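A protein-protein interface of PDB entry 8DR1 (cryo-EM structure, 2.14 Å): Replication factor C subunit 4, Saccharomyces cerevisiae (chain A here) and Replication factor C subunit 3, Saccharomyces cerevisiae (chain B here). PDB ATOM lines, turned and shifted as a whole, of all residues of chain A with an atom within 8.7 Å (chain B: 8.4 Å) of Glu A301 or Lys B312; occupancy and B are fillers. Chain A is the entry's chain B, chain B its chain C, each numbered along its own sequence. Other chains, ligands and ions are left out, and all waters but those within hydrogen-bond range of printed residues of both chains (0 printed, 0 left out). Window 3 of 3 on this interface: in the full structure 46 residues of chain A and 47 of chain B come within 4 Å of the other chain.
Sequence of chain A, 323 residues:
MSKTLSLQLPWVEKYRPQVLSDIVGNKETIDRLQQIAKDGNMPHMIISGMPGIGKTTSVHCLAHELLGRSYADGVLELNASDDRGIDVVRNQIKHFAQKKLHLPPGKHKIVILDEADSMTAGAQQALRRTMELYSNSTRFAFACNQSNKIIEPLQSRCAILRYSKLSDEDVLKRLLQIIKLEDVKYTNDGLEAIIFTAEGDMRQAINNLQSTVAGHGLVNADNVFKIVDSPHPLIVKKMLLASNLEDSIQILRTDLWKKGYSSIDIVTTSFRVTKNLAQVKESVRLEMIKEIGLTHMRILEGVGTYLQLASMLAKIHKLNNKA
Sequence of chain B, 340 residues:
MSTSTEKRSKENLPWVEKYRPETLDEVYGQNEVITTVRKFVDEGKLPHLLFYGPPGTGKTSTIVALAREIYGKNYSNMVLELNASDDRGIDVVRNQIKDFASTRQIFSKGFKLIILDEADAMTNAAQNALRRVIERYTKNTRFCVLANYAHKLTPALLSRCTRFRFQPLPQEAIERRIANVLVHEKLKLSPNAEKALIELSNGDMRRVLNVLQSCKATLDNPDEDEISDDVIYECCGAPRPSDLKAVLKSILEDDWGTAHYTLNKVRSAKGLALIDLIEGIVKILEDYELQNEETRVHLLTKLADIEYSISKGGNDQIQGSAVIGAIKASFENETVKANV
The guanidinium group (NH2) of Arg A298 is in salt-bridge range of the side-chain carboxylate (OD1) of Asp B305 (2.6 Å).
OE1 of Glu A301 sits at hydrogen-bond distance from OH of Tyr B308.
N of Val A303 lies within hydrogen-bond range of O of Arg A298.
O of Tyr B308 sits at hydrogen-bond distance from OG of Ser B311.
Among the printed residues, pairs that only touch across the chains: Arg A298 with Tyr B308, Val A303 with Ser B311, Val A303 with Glu B307 and Glu A301 with Lys B312.
Glu A301 touches just these residues of chain B: Tyr B308 (2.5 Å) and Lys B312 (3.8 Å).
Of chain A, only Glu A301 comes within 4 Å of Lys B312.
Of the printed residues of chain B, Val A303 touches Glu B307 and Ser B311.
Printed residues of chain A within 4 Å of Tyr B308: Arg A298 (3.5 Å) and Glu A301 (2.5 Å).
Printed residues of chain A within 4 Å of Glu B307: Val A303.
Of the printed residues of chain B, Arg A298 touches Asp B305 (2.6 Å) and Tyr B308 (3.5 Å).
Of the printed residues of chain A, Asp B305 touches Arg A298 (2.6 Å).
The nearest residue of chain B that does not touch Glu A301 is Ser B311 (5.1 Å).
The nearest printed residue of chain B that does not touch Val A303 is Tyr B308 (4.3 Å).
Of the 12 printed residues of chain A, 3 touch a printed residue of chain B.
Hydrophobic or aromatic side chains of chain A within 4 Å of the printed part of chain B: Val A303.
Among the printed residues, 6 pairs touch across the chains.
Among the printed residues, Asp or Glu carboxylates within 4 Å of a Lys or Arg side-chain nitrogen of the other chain: Arg A298 with Asp B305.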
ATOM      1  N   ILE A 264     -13.630  -4.709  30.082  1.00  0.00           N
ATOM      2  CA  ILE A 264     -12.556  -3.794  29.706  1.00  0.00           C
ATOM      3  C   ILE A 264     -11.442  -4.548  28.988  1.00  0.00           C
ATOM      4  O   ILE A 264     -10.909  -4.081  27.972  1.00  0.00           O
ATOM      5  CB  ILE A 264     -12.035  -3.047  30.951  1.00  0.00           C
ATOM      6  CG1 ILE A 264     -11.054  -1.941  30.549  1.00  0.00           C
ATOM      7  CG2 ILE A 264     -11.378  -4.011  31.932  1.00  0.00           C
ATOM      8  CD1 ILE A 264     -11.671  -0.846  29.703  1.00  0.00           C
ATOM      9  N   LEU A 294     -16.191   3.816  20.868  1.00  0.00           N
ATOM     10  CA  LEU A 294     -17.458   4.184  21.495  1.00  0.00           C
ATOM     11  C   LEU A 294     -17.783   3.234  22.643  1.00  0.00           C
ATOM     12  O   LEU A 294     -18.107   3.664  23.760  1.00  0.00           O
ATOM     13  CB  LEU A 294     -18.578   4.174  20.454  1.00  0.00           C
ATOM     14  CG  LEU A 294     -19.941   4.678  20.935  1.00  0.00           C
ATOM     15  CD1 LEU A 294     -20.615   5.506  19.852  1.00  0.00           C
ATOM     16  CD2 LEU A 294     -20.836   3.521  21.361  1.00  0.00           C
ATOM     17  N   THR A 295     -17.683   1.927  22.384  1.00  0.00           N
ATOM     18  CA  THR A 295     -17.978   0.951  23.431  1.00  0.00           C
ATOM     19  C   THR A 295     -16.998   1.069  24.595  1.00  0.00           C
ATOM     20  O   THR A 295     -17.385   0.927  25.760  1.00  0.00           O
ATOM     21  CB  THR A 295     -17.956  -0.464  22.852  1.00  0.00           C
ATOM     22  OG1 THR A 295     -19.028  -0.613  21.914  1.00  0.00           O
ATOM     23  CG2 THR A 295     -18.110  -1.502  23.958  1.00  0.00           C
ATOM     24  N   HIS A 296     -15.720   1.315  24.298  1.00  0.00           N
ATOM     25  CA  HIS A 296     -14.717   1.457  25.348  1.00  0.00           C
ATOM     26  C   HIS A 296     -15.019   2.656  26.239  1.00  0.00           C
ATOM     27  O   HIS A 296     -14.910   2.571  27.467  1.00  0.00           O
ATOM     28  CB  HIS A 296     -13.329   1.591  24.718  1.00  0.00           C
ATOM     29  CG  HIS A 296     -12.204   1.549  25.705  1.00  0.00           C
ATOM     30  ND1 HIS A 296     -10.936   1.998  25.405  1.00  0.00           N
ATOM     31  CD2 HIS A 296     -12.155   1.114  26.986  1.00  0.00           C
ATOM     32  CE1 HIS A 296     -10.154   1.841  26.457  1.00  0.00           C
ATOM     33  NE2 HIS A 296     -10.870   1.307  27.431  1.00  0.00           N
ATOM     34  N   MET A 297     -15.398   3.783  25.634  1.00  0.00           N
ATOM     35  CA  MET A 297     -15.763   4.952  26.426  1.00  0.00           C
ATOM     36  C   MET A 297     -16.982   4.661  27.289  1.00  0.00           C
ATOM     37  O   MET A 297     -17.034   5.065  28.456  1.00  0.00           O
ATOM     38  CB  MET A 297     -16.022   6.149  25.513  1.00  0.00           C
ATOM     39  CG  MET A 297     -14.756   6.827  25.017  1.00  0.00           C
ATOM     40  SD  MET A 297     -15.086   8.291  24.022  1.00  0.00           S
ATOM     41  CE  MET A 297     -15.874   7.561  22.589  1.00  0.00           C
ATOM     42  N   ARG A 298     -17.972   3.957  26.736  1.00  0.00           N
ATOM     43  CA  ARG A 298     -19.136   3.598  27.540  1.00  0.00           C
ATOM     44  C   ARG A 298     -18.739   2.722  28.724  1.00  0.00           C
ATOM     45  O   ARG A 298     -19.226   2.920  29.843  1.00  0.00           O
ATOM     46  CB  ARG A 298     -20.179   2.893  26.674  1.00  0.00           C
ATOM     47  CG  ARG A 298     -21.009   3.840  25.825  1.00  0.00           C
ATOM     48  CD  ARG A 298     -22.282   3.183  25.323  1.00  0.00           C
ATOM     49  NE  ARG A 298     -23.034   4.068  24.441  1.00  0.00           N
ATOM     50  CZ  ARG A 298     -23.954   3.664  23.576  1.00  0.00           C
ATOM     51  NH1 ARG A 298     -24.278   2.387  23.453  1.00  0.00           N
ATOM     52  NH2 ARG A 298     -24.564   4.565  22.811  1.00  0.00           N
ATOM     53  N   ILE A 299     -17.855   1.748  28.497  1.00  0.00           N
ATOM     54  CA  ILE A 299     -17.447   0.845  29.571  1.00  0.00           C
ATOM     55  C   ILE A 299     -16.690   1.609  30.653  1.00  0.00           C
ATOM     56  O   ILE A 299     -16.940   1.435  31.851  1.00  0.00           O
ATOM     57  CB  ILE A 299     -16.610  -0.319  29.010  1.00  0.00           C
ATOM     58  CG1 ILE A 299     -17.499  -1.263  28.197  1.00  0.00           C
ATOM     59  CG2 ILE A 299     -15.922  -1.076  30.141  1.00  0.00           C
ATOM     60  CD1 ILE A 299     -16.733  -2.235  27.328  1.00  0.00           C
ATOM     61  N   LEU A 300     -15.749   2.466  30.247  1.00  0.00           N
ATOM     62  CA  LEU A 300     -15.016   3.263  31.227  1.00  0.00           C
ATOM     63  C   LEU A 300     -15.953   4.135  32.048  1.00  0.00           C
ATOM     64  O   LEU A 300     -15.667   4.431  33.214  1.00  0.00           O
ATOM     65  CB  LEU A 300     -13.967   4.133  30.533  1.00  0.00           C
ATOM     66  CG  LEU A 300     -12.711   3.427  30.016  1.00  0.00           C
ATOM     67  CD1 LEU A 300     -11.869   4.387  29.190  1.00  0.00           C
ATOM     68  CD2 LEU A 300     -11.894   2.851  31.164  1.00  0.00           C
ATOM     69  N   GLU A 301     -17.073   4.560  31.460  1.00  0.00           N
ATOM     70  CA  GLU A 301     -18.041   5.367  32.192  1.00  0.00           C
ATOM     71  C   GLU A 301     -18.705   4.583  33.314  1.00  0.00           C
ATOM     72  O   GLU A 301     -19.295   5.189  34.215  1.00  0.00           O
ATOM     73  CB  GLU A 301     -19.105   5.900  31.231  1.00  0.00           C
ATOM     74  CG  GLU A 301     -19.363   7.390  31.354  1.00  0.00           C
ATOM     75  CD  GLU A 301     -20.284   7.912  30.272  1.00  0.00           C
ATOM     76  OE1 GLU A 301     -19.895   7.861  29.087  1.00  0.00           O
ATOM     77  OE2 GLU A 301     -21.396   8.375  30.604  1.00  0.00           O
ATOM     78  N   GLY A 302     -18.632   3.254  33.275  1.00  0.00           N
ATOM     79  CA  GLY A 302     -19.214   2.397  34.291  1.00  0.00           C
ATOM     80  C   GLY A 302     -20.221   1.398  33.762  1.00  0.00           C
ATOM     81  O   GLY A 302     -20.564   0.446  34.477  1.00  0.00           O
ATOM     82  N   VAL A 303     -20.711   1.577  32.538  1.00  0.00           N
ATOM     83  CA  VAL A 303     -21.701   0.649  31.963  1.00  0.00           C
ATOM     84  C   VAL A 303     -20.900  -0.445  31.269  1.00  0.00           C
ATOM     85  O   VAL A 303     -20.699  -0.453  30.052  1.00  0.00           O
ATOM     86  CB  VAL A 303     -22.678   1.360  31.022  1.00  0.00           C
ATOM     87  CG1 VAL A 303     -23.904   0.491  30.770  1.00  0.00           C
ATOM     88  CG2 VAL A 303     -23.082   2.712  31.596  1.00  0.00           C
ATOM     89  N   GLY A 304     -20.440  -1.405  32.066  1.00  0.00           N
ATOM     90  CA  GLY A 304     -19.768  -2.576  31.540  1.00  0.00           C
ATOM     91  C   GLY A 304     -20.667  -3.790  31.616  1.00  0.00           C
ATOM     92  O   GLY A 304     -20.776  -4.422  32.670  1.00  0.00           O
ATOM     93  N   ASP B 305     -28.315   1.547  23.584  1.00  0.00           N
ATOM     94  CA  ASP B 305     -28.445   2.998  23.688  1.00  0.00           C
ATOM     95  C   ASP B 305     -29.361   3.382  24.844  1.00  0.00           C
ATOM     96  O   ASP B 305     -29.067   4.319  25.597  1.00  0.00           O
ATOM     97  CB  ASP B 305     -28.974   3.575  22.375  1.00  0.00           C
ATOM     98  CG  ASP B 305     -27.925   3.597  21.281  1.00  0.00           C
ATOM     99  OD1 ASP B 305     -26.738   3.821  21.594  1.00  0.00           O
ATOM    100  OD2 ASP B 305     -28.289   3.390  20.104  1.00  0.00           O
ATOM    101  N   ILE B 306     -30.478   2.669  25.000  1.00  0.00           N
ATOM    102  CA  ILE B 306     -31.415   2.981  26.076  1.00  0.00           C
ATOM    103  C   ILE B 306     -30.766   2.747  27.437  1.00  0.00           C
ATOM    104  O   ILE B 306     -30.939   3.543  28.366  1.00  0.00           O
ATOM    105  CB  ILE B 306     -32.708   2.162  25.916  1.00  0.00           C
ATOM    106  CG1 ILE B 306     -33.486   2.640  24.686  1.00  0.00           C
ATOM    107  CG2 ILE B 306     -33.564   2.272  27.174  1.00  0.00           C
ATOM    108  CD1 ILE B 306     -34.637   1.738  24.293  1.00  0.00           C
ATOM    109  N   GLU B 307     -30.026   1.644  27.583  1.00  0.00           N
ATOM    110  CA  GLU B 307     -29.353   1.379  28.851  1.00  0.00           C
ATOM    111  C   GLU B 307     -28.332   2.466  29.164  1.00  0.00           C
ATOM    112  O   GLU B 307     -28.241   2.936  30.306  1.00  0.00           O
ATOM    113  CB  GLU B 307     -28.684   0.001  28.816  1.00  0.00           C
ATOM    114  CG  GLU B 307     -27.696  -0.249  29.955  1.00  0.00           C
ATOM    115  CD  GLU B 307     -27.092  -1.642  29.916  1.00  0.00           C
ATOM    116  OE1 GLU B 307     -27.563  -2.514  30.676  1.00  0.00           O
ATOM    117  OE2 GLU B 307     -26.145  -1.863  29.134  1.00  0.00           O
ATOM    118  N   TYR B 308     -27.558   2.883  28.158  1.00  0.00           N
ATOM    119  CA  TYR B 308     -26.588   3.949  28.380  1.00  0.00           C
ATOM    120  C   TYR B 308     -27.281   5.239  28.797  1.00  0.00           C
ATOM    121  O   TYR B 308     -26.809   5.946  29.695  1.00  0.00           O
ATOM    122  CB  TYR B 308     -25.751   4.171  27.122  1.00  0.00           C
ATOM    123  CG  TYR B 308     -24.715   5.260  27.271  1.00  0.00           C
ATOM    124  CD1 TYR B 308     -23.623   5.096  28.113  1.00  0.00           C
ATOM    125  CD2 TYR B 308     -24.828   6.453  26.570  1.00  0.00           C
ATOM    126  CE1 TYR B 308     -22.674   6.089  28.254  1.00  0.00           C
ATOM    127  CE2 TYR B 308     -23.884   7.451  26.704  1.00  0.00           C
ATOM    128  CZ  TYR B 308     -22.808   7.264  27.546  1.00  0.00           C
ATOM    129  OH  TYR B 308     -21.868   8.258  27.677  1.00  0.00           O
ATOM    130  N   SER B 309     -28.406   5.566  28.156  1.00  0.00           N
ATOM    131  CA  SER B 309     -29.148   6.763  28.538  1.00  0.00           C
ATOM    132  C   SER B 309     -29.650   6.664  29.974  1.00  0.00           C
ATOM    133  O   SER B 309     -29.570   7.633  30.738  1.00  0.00           O
ATOM    134  CB  SER B 309     -30.314   6.987  27.576  1.00  0.00           C
ATOM    135  OG  SER B 309     -31.147   8.039  28.025  1.00  0.00           O
ATOM    136  N   ILE B 310     -30.168   5.496  30.359  1.00  0.00           N
ATOM    137  CA  ILE B 310     -30.652   5.308  31.724  1.00  0.00           C
ATOM    138  C   ILE B 310     -29.517   5.498  32.720  1.00  0.00           C
ATOM    139  O   ILE B 310     -29.717   6.034  33.817  1.00  0.00           O
ATOM    140  CB  ILE B 310     -31.311   3.924  31.878  1.00  0.00           C
ATOM    141  CG1 ILE B 310     -32.674   3.903  31.184  1.00  0.00           C
ATOM    142  CG2 ILE B 310     -31.452   3.558  33.351  1.00  0.00           C
ATOM    143  CD1 ILE B 310     -33.185   2.509  30.882  1.00  0.00           C
ATOM    144  N   SER B 311     -28.309   5.062  32.358  1.00  0.00           N
ATOM    145  CA  SER B 311     -27.190   5.155  33.291  1.00  0.00           C
ATOM    146  C   SER B 311     -26.935   6.593  33.732  1.00  0.00           C
ATOM    147  O   SER B 311     -26.356   6.818  34.800  1.00  0.00           O
ATOM    148  CB  SER B 311     -25.927   4.564  32.662  1.00  0.00           C
ATOM    149  OG  SER B 311     -25.380   5.439  31.692  1.00  0.00           O
ATOM    150  N   LYS B 312     -27.355   7.575  32.934  1.00  0.00           N
ATOM    151  CA  LYS B 312     -27.175   8.984  33.263  1.00  0.00           C
ATOM    152  C   LYS B 312     -28.445   9.639  33.796  1.00  0.00           C
ATOM    153  O   LYS B 312     -28.467  10.861  33.978  1.00  0.00           O
ATOM    154  CB  LYS B 312     -26.683   9.754  32.035  1.00  0.00           C
ATOM    155  CG  LYS B 312     -25.317   9.323  31.539  1.00  0.00           C
ATOM    156  CD  LYS B 312     -24.777  10.292  30.500  1.00  0.00           C
ATOM    157  CE  LYS B 312     -24.672   9.633  29.142  1.00  0.00           C
ATOM    158  NZ  LYS B 312     -26.005   9.247  28.598  1.00  0.00           N
ATOM    159  N   GLY B 313     -29.491   8.868  34.053  1.00  0.00           N
ATOM    160  CA  GLY B 313     -30.752   9.418  34.523  1.00  0.00           C
ATOM    161  C   GLY B 313     -31.755   9.558  33.384  1.00  0.00           C
ATOM    162  O   GLY B 313     -31.975   8.616  32.625  1.00  0.00           O
ATOM    163  N   GLY B 314     -32.359  10.735  33.274  1.00  0.00           N
ATOM    164  CA  GLY B 314     -33.304  11.016  32.210  1.00  0.00           C
ATOM    165  C   GLY B 314     -34.742  10.769  32.621  1.00  0.00           C
ATOM    166  O   GLY B 314     -35.063  10.460  33.772  1.00  0.00           O
ATOM    167  N   ASN B 315     -35.625  10.911  31.634  1.00  0.00           N
ATOM    168  CA  ASN B 315     -37.062  10.774  31.838  1.00  0.00           C
ATOM    169  C   ASN B 315     -37.448   9.301  31.742  1.00  0.00           C
ATOM    170  O   ASN B 315     -37.269   8.672  30.695  1.00  0.00           O
ATOM    171  CB  ASN B 315     -37.825  11.607  30.808  1.00  0.00           C
ATOM    172  CG  ASN B 315     -39.315  11.671  31.088  1.00  0.00           C
ATOM    173  OD1 ASN B 315     -39.922  10.695  31.526  1.00  0.00           O
ATOM    174  ND2 ASN B 315     -39.913  12.829  30.833  1.00  0.00           N
ATOM    175  N   GLN B 319     -38.185   6.804  28.400  1.00  0.00           N
ATOM    176  CA  GLN B 319     -37.322   5.640  28.214  1.00  0.00           C
ATOM    177  C   GLN B 319     -38.139   4.358  28.065  1.00  0.00           C
ATOM    178  O   GLN B 319     -37.815   3.502  27.232  1.00  0.00           O
ATOM    179  CB  GLN B 319     -36.341   5.538  29.381  1.00  0.00           C
ATOM    180  CG  GLN B 319     -35.279   6.632  29.365  1.00  0.00           C
ATOM    181  CD  GLN B 319     -34.578   6.805  30.700  1.00  0.00           C
ATOM    182  OE1 GLN B 319     -35.000   6.253  31.715  1.00  0.00           O
ATOM    183  NE2 GLN B 319     -33.503   7.582  30.703  1.00  0.00           N
